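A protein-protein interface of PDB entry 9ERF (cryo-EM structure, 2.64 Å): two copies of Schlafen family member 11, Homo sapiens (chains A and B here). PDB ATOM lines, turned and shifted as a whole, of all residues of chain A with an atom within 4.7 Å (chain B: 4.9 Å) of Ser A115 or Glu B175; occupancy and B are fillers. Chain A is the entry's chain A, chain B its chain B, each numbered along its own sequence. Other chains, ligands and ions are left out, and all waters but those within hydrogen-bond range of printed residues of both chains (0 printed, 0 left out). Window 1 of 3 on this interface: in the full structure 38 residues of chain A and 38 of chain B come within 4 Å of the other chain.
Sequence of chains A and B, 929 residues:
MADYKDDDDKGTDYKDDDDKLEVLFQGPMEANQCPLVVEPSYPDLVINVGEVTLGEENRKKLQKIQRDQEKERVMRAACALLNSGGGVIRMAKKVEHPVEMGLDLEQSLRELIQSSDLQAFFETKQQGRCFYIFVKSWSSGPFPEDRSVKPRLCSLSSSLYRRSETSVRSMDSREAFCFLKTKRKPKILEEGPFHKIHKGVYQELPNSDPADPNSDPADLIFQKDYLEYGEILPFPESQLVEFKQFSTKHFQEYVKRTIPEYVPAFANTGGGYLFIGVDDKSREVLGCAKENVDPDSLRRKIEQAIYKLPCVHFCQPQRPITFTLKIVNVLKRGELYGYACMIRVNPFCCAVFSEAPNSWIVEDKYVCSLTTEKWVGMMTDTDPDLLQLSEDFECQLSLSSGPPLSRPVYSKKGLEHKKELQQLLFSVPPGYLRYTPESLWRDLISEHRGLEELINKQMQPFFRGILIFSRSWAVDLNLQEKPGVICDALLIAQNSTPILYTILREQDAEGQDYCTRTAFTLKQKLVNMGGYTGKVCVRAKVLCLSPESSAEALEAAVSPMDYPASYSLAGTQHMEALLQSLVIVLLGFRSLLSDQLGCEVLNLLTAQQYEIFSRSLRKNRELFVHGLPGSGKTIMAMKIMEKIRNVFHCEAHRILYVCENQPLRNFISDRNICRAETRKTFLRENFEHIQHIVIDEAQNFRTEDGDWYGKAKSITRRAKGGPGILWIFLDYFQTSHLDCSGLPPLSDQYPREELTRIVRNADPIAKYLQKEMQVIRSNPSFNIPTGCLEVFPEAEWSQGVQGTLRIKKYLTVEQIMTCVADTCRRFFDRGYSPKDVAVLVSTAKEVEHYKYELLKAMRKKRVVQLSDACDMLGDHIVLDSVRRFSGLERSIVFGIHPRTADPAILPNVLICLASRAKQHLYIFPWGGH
N of Ser A115 lies within hydrogen-bond range of O of Arg A110, 3.1 Å away. OG of Ser A115 sits at hydrogen-bond distance from N of Asp A117. The guanidinium group (NH1) of Arg B162 lies within salt-bridge range of the side-chain carboxylate (OE1) of Glu B175, 2.4 Å away. OD1 of Asp B172 lies within hydrogen-bond range of N of Glu B175 (2.6 Å).
Of the 11 printed residues of chain B, 2 touch a printed residue of chain A. Of the 6 printed residues of chain A, 3 touch a printed residue of chain B.
The side-chain carboxylate (OE1) of Glu B175 lies within hydrogen-bond range of the side-chain hydroxyl (OG) of Ser A115, at 3.5 Å. The side-chain hydroxyl (OG) of Ser A116 sits close to the guanidinium group (NH1) of Arg B162. The side-chain carboxylate (OE1) of Glu B175 lies within hydrogen-bond range of the side-chain hydroxyl (OG) of Ser A116.
Ser A115 touches one residue of chain B. Glu B175 touches just these residues of chain A: Ser A115 and Ser A116. Of the printed residues of chain B, Asp A117 touches Arg B162. Of the printed residues of chain B, Ser A116 touches Arg B162 and Glu B175. Of the printed residues of chain A, Arg B162 touches Ser A116 and Asp A117. Ser B170 touches none of the printed residues of chain A.
Among the printed residues, pairs that only touch across the chains: Asp A117 with Arg B162 (3.8 Å).
No position is printed for both chains.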
ATOM      1  N   ARG A 110      -9.609   2.348  31.951  1.00  0.00           N
ATOM      2  CA  ARG A 110      -8.762   1.271  31.454  1.00  0.00           C
ATOM      3  C   ARG A 110      -8.934   0.012  32.285  1.00  0.00           C
ATOM      4  O   ARG A 110      -9.009  -1.090  31.741  1.00  0.00           O
ATOM      5  CB  ARG A 110      -7.298   1.696  31.465  1.00  0.00           C
ATOM      6  CG  ARG A 110      -6.903   2.584  30.327  1.00  0.00           C
ATOM      7  CD  ARG A 110      -5.407   2.773  30.276  1.00  0.00           C
ATOM      8  NE  ARG A 110      -5.076   4.034  29.630  1.00  0.00           N
ATOM      9  CZ  ARG A 110      -4.805   5.161  30.271  1.00  0.00           C
ATOM     10  NH1 ARG A 110      -4.719   5.208  31.587  1.00  0.00           N
ATOM     11  NH2 ARG A 110      -4.618   6.272  29.570  1.00  0.00           N
ATOM     12  N   ILE A 113     -12.399  -1.682  31.482  1.00  0.00           N
ATOM     13  CA  ILE A 113     -12.471  -2.498  30.269  1.00  0.00           C
ATOM     14  C   ILE A 113     -11.278  -3.434  30.108  1.00  0.00           C
ATOM     15  O   ILE A 113     -11.182  -4.123  29.083  1.00  0.00           O
ATOM     16  CB  ILE A 113     -12.608  -1.625  29.003  1.00  0.00           C
ATOM     17  CG1 ILE A 113     -11.459  -0.623  28.898  1.00  0.00           C
ATOM     18  CG2 ILE A 113     -13.952  -0.922  28.998  1.00  0.00           C
ATOM     19  CD1 ILE A 113     -11.232  -0.103  27.511  1.00  0.00           C
ATOM     20  N   GLN A 114     -10.374  -3.489  31.086  1.00  0.00           N
ATOM     21  CA  GLN A 114      -9.206  -4.369  31.049  1.00  0.00           C
ATOM     22  C   GLN A 114      -8.412  -4.197  29.760  1.00  0.00           C
ATOM     23  O   GLN A 114      -7.975  -5.169  29.142  1.00  0.00           O
ATOM     24  CB  GLN A 114      -9.606  -5.830  31.223  1.00  0.00           C
ATOM     25  CG  GLN A 114     -10.484  -6.116  32.407  1.00  0.00           C
ATOM     26  CD  GLN A 114     -10.980  -7.538  32.390  1.00  0.00           C
ATOM     27  OE1 GLN A 114     -10.301  -8.446  32.865  1.00  0.00           O
ATOM     28  NE2 GLN A 114     -12.152  -7.750  31.806  1.00  0.00           N
ATOM     29  N   SER A 115      -8.212  -2.951  29.350  1.00  0.00           N
ATOM     30  CA  SER A 115      -7.536  -2.690  28.091  1.00  0.00           C
ATOM     31  C   SER A 115      -7.162  -1.221  28.025  1.00  0.00           C
ATOM     32  O   SER A 115      -7.820  -0.373  28.627  1.00  0.00           O
ATOM     33  CB  SER A 115      -8.419  -3.067  26.897  1.00  0.00           C
ATOM     34  OG  SER A 115      -7.753  -2.844  25.670  1.00  0.00           O
ATOM     35  N   SER A 116      -6.097  -0.934  27.284  1.00  0.00           N
ATOM     36  CA  SER A 116      -5.713   0.442  27.012  1.00  0.00           C
ATOM     37  C   SER A 116      -6.413   1.009  25.787  1.00  0.00           C
ATOM     38  O   SER A 116      -6.208   2.184  25.468  1.00  0.00           O
ATOM     39  CB  SER A 116      -4.198   0.538  26.836  1.00  0.00           C
ATOM     40  OG  SER A 116      -3.757  -0.246  25.747  1.00  0.00           O
ATOM     41  N   ASP A 117      -7.231   0.211  25.100  1.00  0.00           N
ATOM     42  CA  ASP A 117      -7.979   0.671  23.932  1.00  0.00           C
ATOM     43  C   ASP A 117      -9.261   1.375  24.378  1.00  0.00           C
ATOM     44  O   ASP A 117     -10.375   0.876  24.232  1.00  0.00           O
ATOM     45  CB  ASP A 117      -8.280  -0.500  23.008  1.00  0.00           C
ATOM     46  CG  ASP A 117      -8.634  -0.061  21.602  1.00  0.00           C
ATOM     47  OD1 ASP A 117      -8.470   1.133  21.285  1.00  0.00           O
ATOM     48  OD2 ASP A 117      -9.080  -0.914  20.811  1.00  0.00           O
ATOM     49  N   ARG B 162       0.340   1.844  22.324  1.00  0.00           N
ATOM     50  CA  ARG B 162      -0.781   2.523  21.780  1.00  0.00           C
ATOM     51  C   ARG B 162      -1.041   3.815  22.503  1.00  0.00           C
ATOM     52  O   ARG B 162      -0.754   3.920  23.634  1.00  0.00           O
ATOM     53  CB  ARG B 162      -1.996   1.653  21.894  1.00  0.00           C
ATOM     54  CG  ARG B 162      -2.550   1.410  23.264  1.00  0.00           C
ATOM     55  CD  ARG B 162      -4.034   1.160  23.161  1.00  0.00           C
ATOM     56  NE  ARG B 162      -4.419   0.508  21.927  1.00  0.00           N
ATOM     57  CZ  ARG B 162      -4.718  -0.775  21.805  1.00  0.00           C
ATOM     58  NH1 ARG B 162      -4.675  -1.574  22.841  1.00  0.00           N
ATOM     59  NH2 ARG B 162      -5.062  -1.260  20.634  1.00  0.00           N
ATOM     60  N   SER B 170       1.899   0.313  26.935  1.00  0.00           N
ATOM     61  CA  SER B 170       2.349  -0.876  26.230  1.00  0.00           C
ATOM     62  C   SER B 170       1.264  -1.939  26.252  1.00  0.00           C
ATOM     63  O   SER B 170       0.536  -2.086  27.236  1.00  0.00           O
ATOM     64  CB  SER B 170       3.626  -1.426  26.858  1.00  0.00           C
ATOM     65  OG  SER B 170       3.449  -1.664  28.239  1.00  0.00           O
ATOM     66  N   MET B 171       1.151  -2.675  25.155  1.00  0.00           N
ATOM     67  CA  MET B 171       0.199  -3.768  25.072  1.00  0.00           C
ATOM     68  C   MET B 171       0.779  -5.010  25.734  1.00  0.00           C
ATOM     69  O   MET B 171       1.923  -5.389  25.467  1.00  0.00           O
ATOM     70  CB  MET B 171      -0.140  -4.064  23.613  1.00  0.00           C
ATOM     71  CG  MET B 171      -0.809  -2.923  22.879  1.00  0.00           C
ATOM     72  SD  MET B 171      -1.064  -3.313  21.144  1.00  0.00           S
ATOM     73  CE  MET B 171      -0.831  -1.712  20.391  1.00  0.00           C
ATOM     74  N   ASP B 172      -0.004  -5.638  26.605  1.00  0.00           N
ATOM     75  CA  ASP B 172       0.369  -6.941  27.123  1.00  0.00           C
ATOM     76  C   ASP B 172       0.258  -7.980  26.010  1.00  0.00           C
ATOM     77  O   ASP B 172      -0.029  -7.659  24.859  1.00  0.00           O
ATOM     78  CB  ASP B 172      -0.505  -7.318  28.320  1.00  0.00           C
ATOM     79  CG  ASP B 172      -1.988  -7.227  28.018  1.00  0.00           C
ATOM     80  OD1 ASP B 172      -2.471  -7.972  27.143  1.00  0.00           O
ATOM     81  OD2 ASP B 172      -2.677  -6.419  28.669  1.00  0.00           O
ATOM     82  N   SER B 173       0.516  -9.243  26.351  1.00  0.00           N
ATOM     83  CA  SER B 173       0.473 -10.287  25.331  1.00  0.00           C
ATOM     84  C   SER B 173      -0.913 -10.397  24.712  1.00  0.00           C
ATOM     85  O   SER B 173      -1.047 -10.481  23.489  1.00  0.00           O
ATOM     86  CB  SER B 173       0.900 -11.627  25.922  1.00  0.00           C
ATOM     87  OG  SER B 173       2.207 -11.555  26.454  1.00  0.00           O
ATOM     88  N   ARG B 174      -1.957 -10.386  25.540  1.00  0.00           N
ATOM     89  CA  ARG B 174      -3.321 -10.493  25.032  1.00  0.00           C
ATOM     90  C   ARG B 174      -3.698  -9.280  24.184  1.00  0.00           C
ATOM     91  O   ARG B 174      -4.303  -9.420  23.110  1.00  0.00           O
ATOM     92  CB  ARG B 174      -4.273 -10.645  26.214  1.00  0.00           C
ATOM     93  CG  ARG B 174      -5.585 -11.314  25.907  1.00  0.00           C
ATOM     94  CD  ARG B 174      -6.460 -11.325  27.143  1.00  0.00           C
ATOM     95  NE  ARG B 174      -6.025 -12.326  28.113  1.00  0.00           N
ATOM     96  CZ  ARG B 174      -5.614 -12.069  29.350  1.00  0.00           C
ATOM     97  NH1 ARG B 174      -5.506 -10.832  29.807  1.00  0.00           N
ATOM     98  NH2 ARG B 174      -5.295 -13.082  30.149  1.00  0.00           N
ATOM     99  N   GLU B 175      -3.348  -8.082  24.653  1.00  0.00           N
ATOM    100  CA  GLU B 175      -3.655  -6.863  23.915  1.00  0.00           C
ATOM    101  C   GLU B 175      -2.950  -6.849  22.568  1.00  0.00           C
ATOM    102  O   GLU B 175      -3.553  -6.517  21.542  1.00  0.00           O
ATOM    103  CB  GLU B 175      -3.235  -5.650  24.741  1.00  0.00           C
ATOM    104  CG  GLU B 175      -4.301  -5.102  25.652  1.00  0.00           C
ATOM    105  CD  GLU B 175      -4.174  -3.609  25.843  1.00  0.00           C
ATOM    106  OE1 GLU B 175      -4.354  -2.862  24.860  1.00  0.00           O
ATOM    107  OE2 GLU B 175      -3.876  -3.184  26.978  1.00  0.00           O
ATOM    108  N   ALA B 176      -1.664  -7.203  22.555  1.00  0.00           N
ATOM    109  CA  ALA B 176      -0.911  -7.248  21.307  1.00  0.00           C
ATOM    110  C   ALA B 176      -1.447  -8.330  20.387  1.00  0.00           C
ATOM    111  O   ALA B 176      -1.462  -8.163  19.166  1.00  0.00           O
ATOM    112  CB  ALA B 176       0.569  -7.481  21.600  1.00  0.00           C
ATOM    113  N   PHE B 177      -1.882  -9.453  20.955  1.00  0.00           N
ATOM    114  CA  PHE B 177      -2.472 -10.514  20.153  1.00  0.00           C
ATOM    115  C   PHE B 177      -3.701 -10.004  19.416  1.00  0.00           C
ATOM    116  O   PHE B 177      -3.819 -10.162  18.196  1.00  0.00           O
ATOM    117  CB  PHE B 177      -2.815 -11.692  21.063  1.00  0.00           C
ATOM    118  CG  PHE B 177      -3.388 -12.875  20.350  1.00  0.00           C
ATOM    119  CD1 PHE B 177      -2.620 -13.604  19.463  1.00  0.00           C
ATOM    120  CD2 PHE B 177      -4.686 -13.279  20.588  1.00  0.00           C
ATOM    121  CE1 PHE B 177      -3.143 -14.698  18.815  1.00  0.00           C
ATOM    122  CE2 PHE B 177      -5.211 -14.374  19.941  1.00  0.00           C
ATOM    123  CZ  PHE B 177      -4.437 -15.084  19.055  1.00  0.00           C
ATOM    124  N   CYS B 178      -4.611  -9.351  20.140  1.00  0.00           N
ATOM    125  CA  CYS B 178      -5.800  -8.795  19.498  1.00  0.00           C
ATOM    126  C   CYS B 178      -5.437  -7.709  18.487  1.00  0.00           C
ATOM    127  O   CYS B 178      -6.032  -7.633  17.407  1.00  0.00           O
ATOM    128  CB  CYS B 178      -6.753  -8.247  20.556  1.00  0.00           C
ATOM    129  SG  CYS B 178      -7.441  -9.519  21.633  1.00  0.00           S
ATOM    130  N   PHE B 179      -4.462  -6.863  18.820  1.00  0.00           N
ATOM    131  CA  PHE B 179      -4.085  -5.766  17.936  1.00  0.00           C
ATOM    132  C   PHE B 179      -3.511  -6.284  16.621  1.00  0.00           C
ATOM    133  O   PHE B 179      -3.885  -5.818  15.538  1.00  0.00           O
ATOM    134  CB  PHE B 179      -3.079  -4.869  18.658  1.00  0.00           C
ATOM    135  CG  PHE B 179      -2.379  -3.894  17.766  1.00  0.00           C
ATOM    136  CD1 PHE B 179      -2.981  -2.703  17.415  1.00  0.00           C
ATOM    137  CD2 PHE B 179      -1.109  -4.164  17.291  1.00  0.00           C
ATOM    138  CE1 PHE B 179      -2.335  -1.808  16.598  1.00  0.00           C
ATOM    139  CE2 PHE B 179      -0.463  -3.268  16.474  1.00  0.00           C
ATOM    140  CZ  PHE B 179      -1.074  -2.090  16.130  1.00  0.00           C
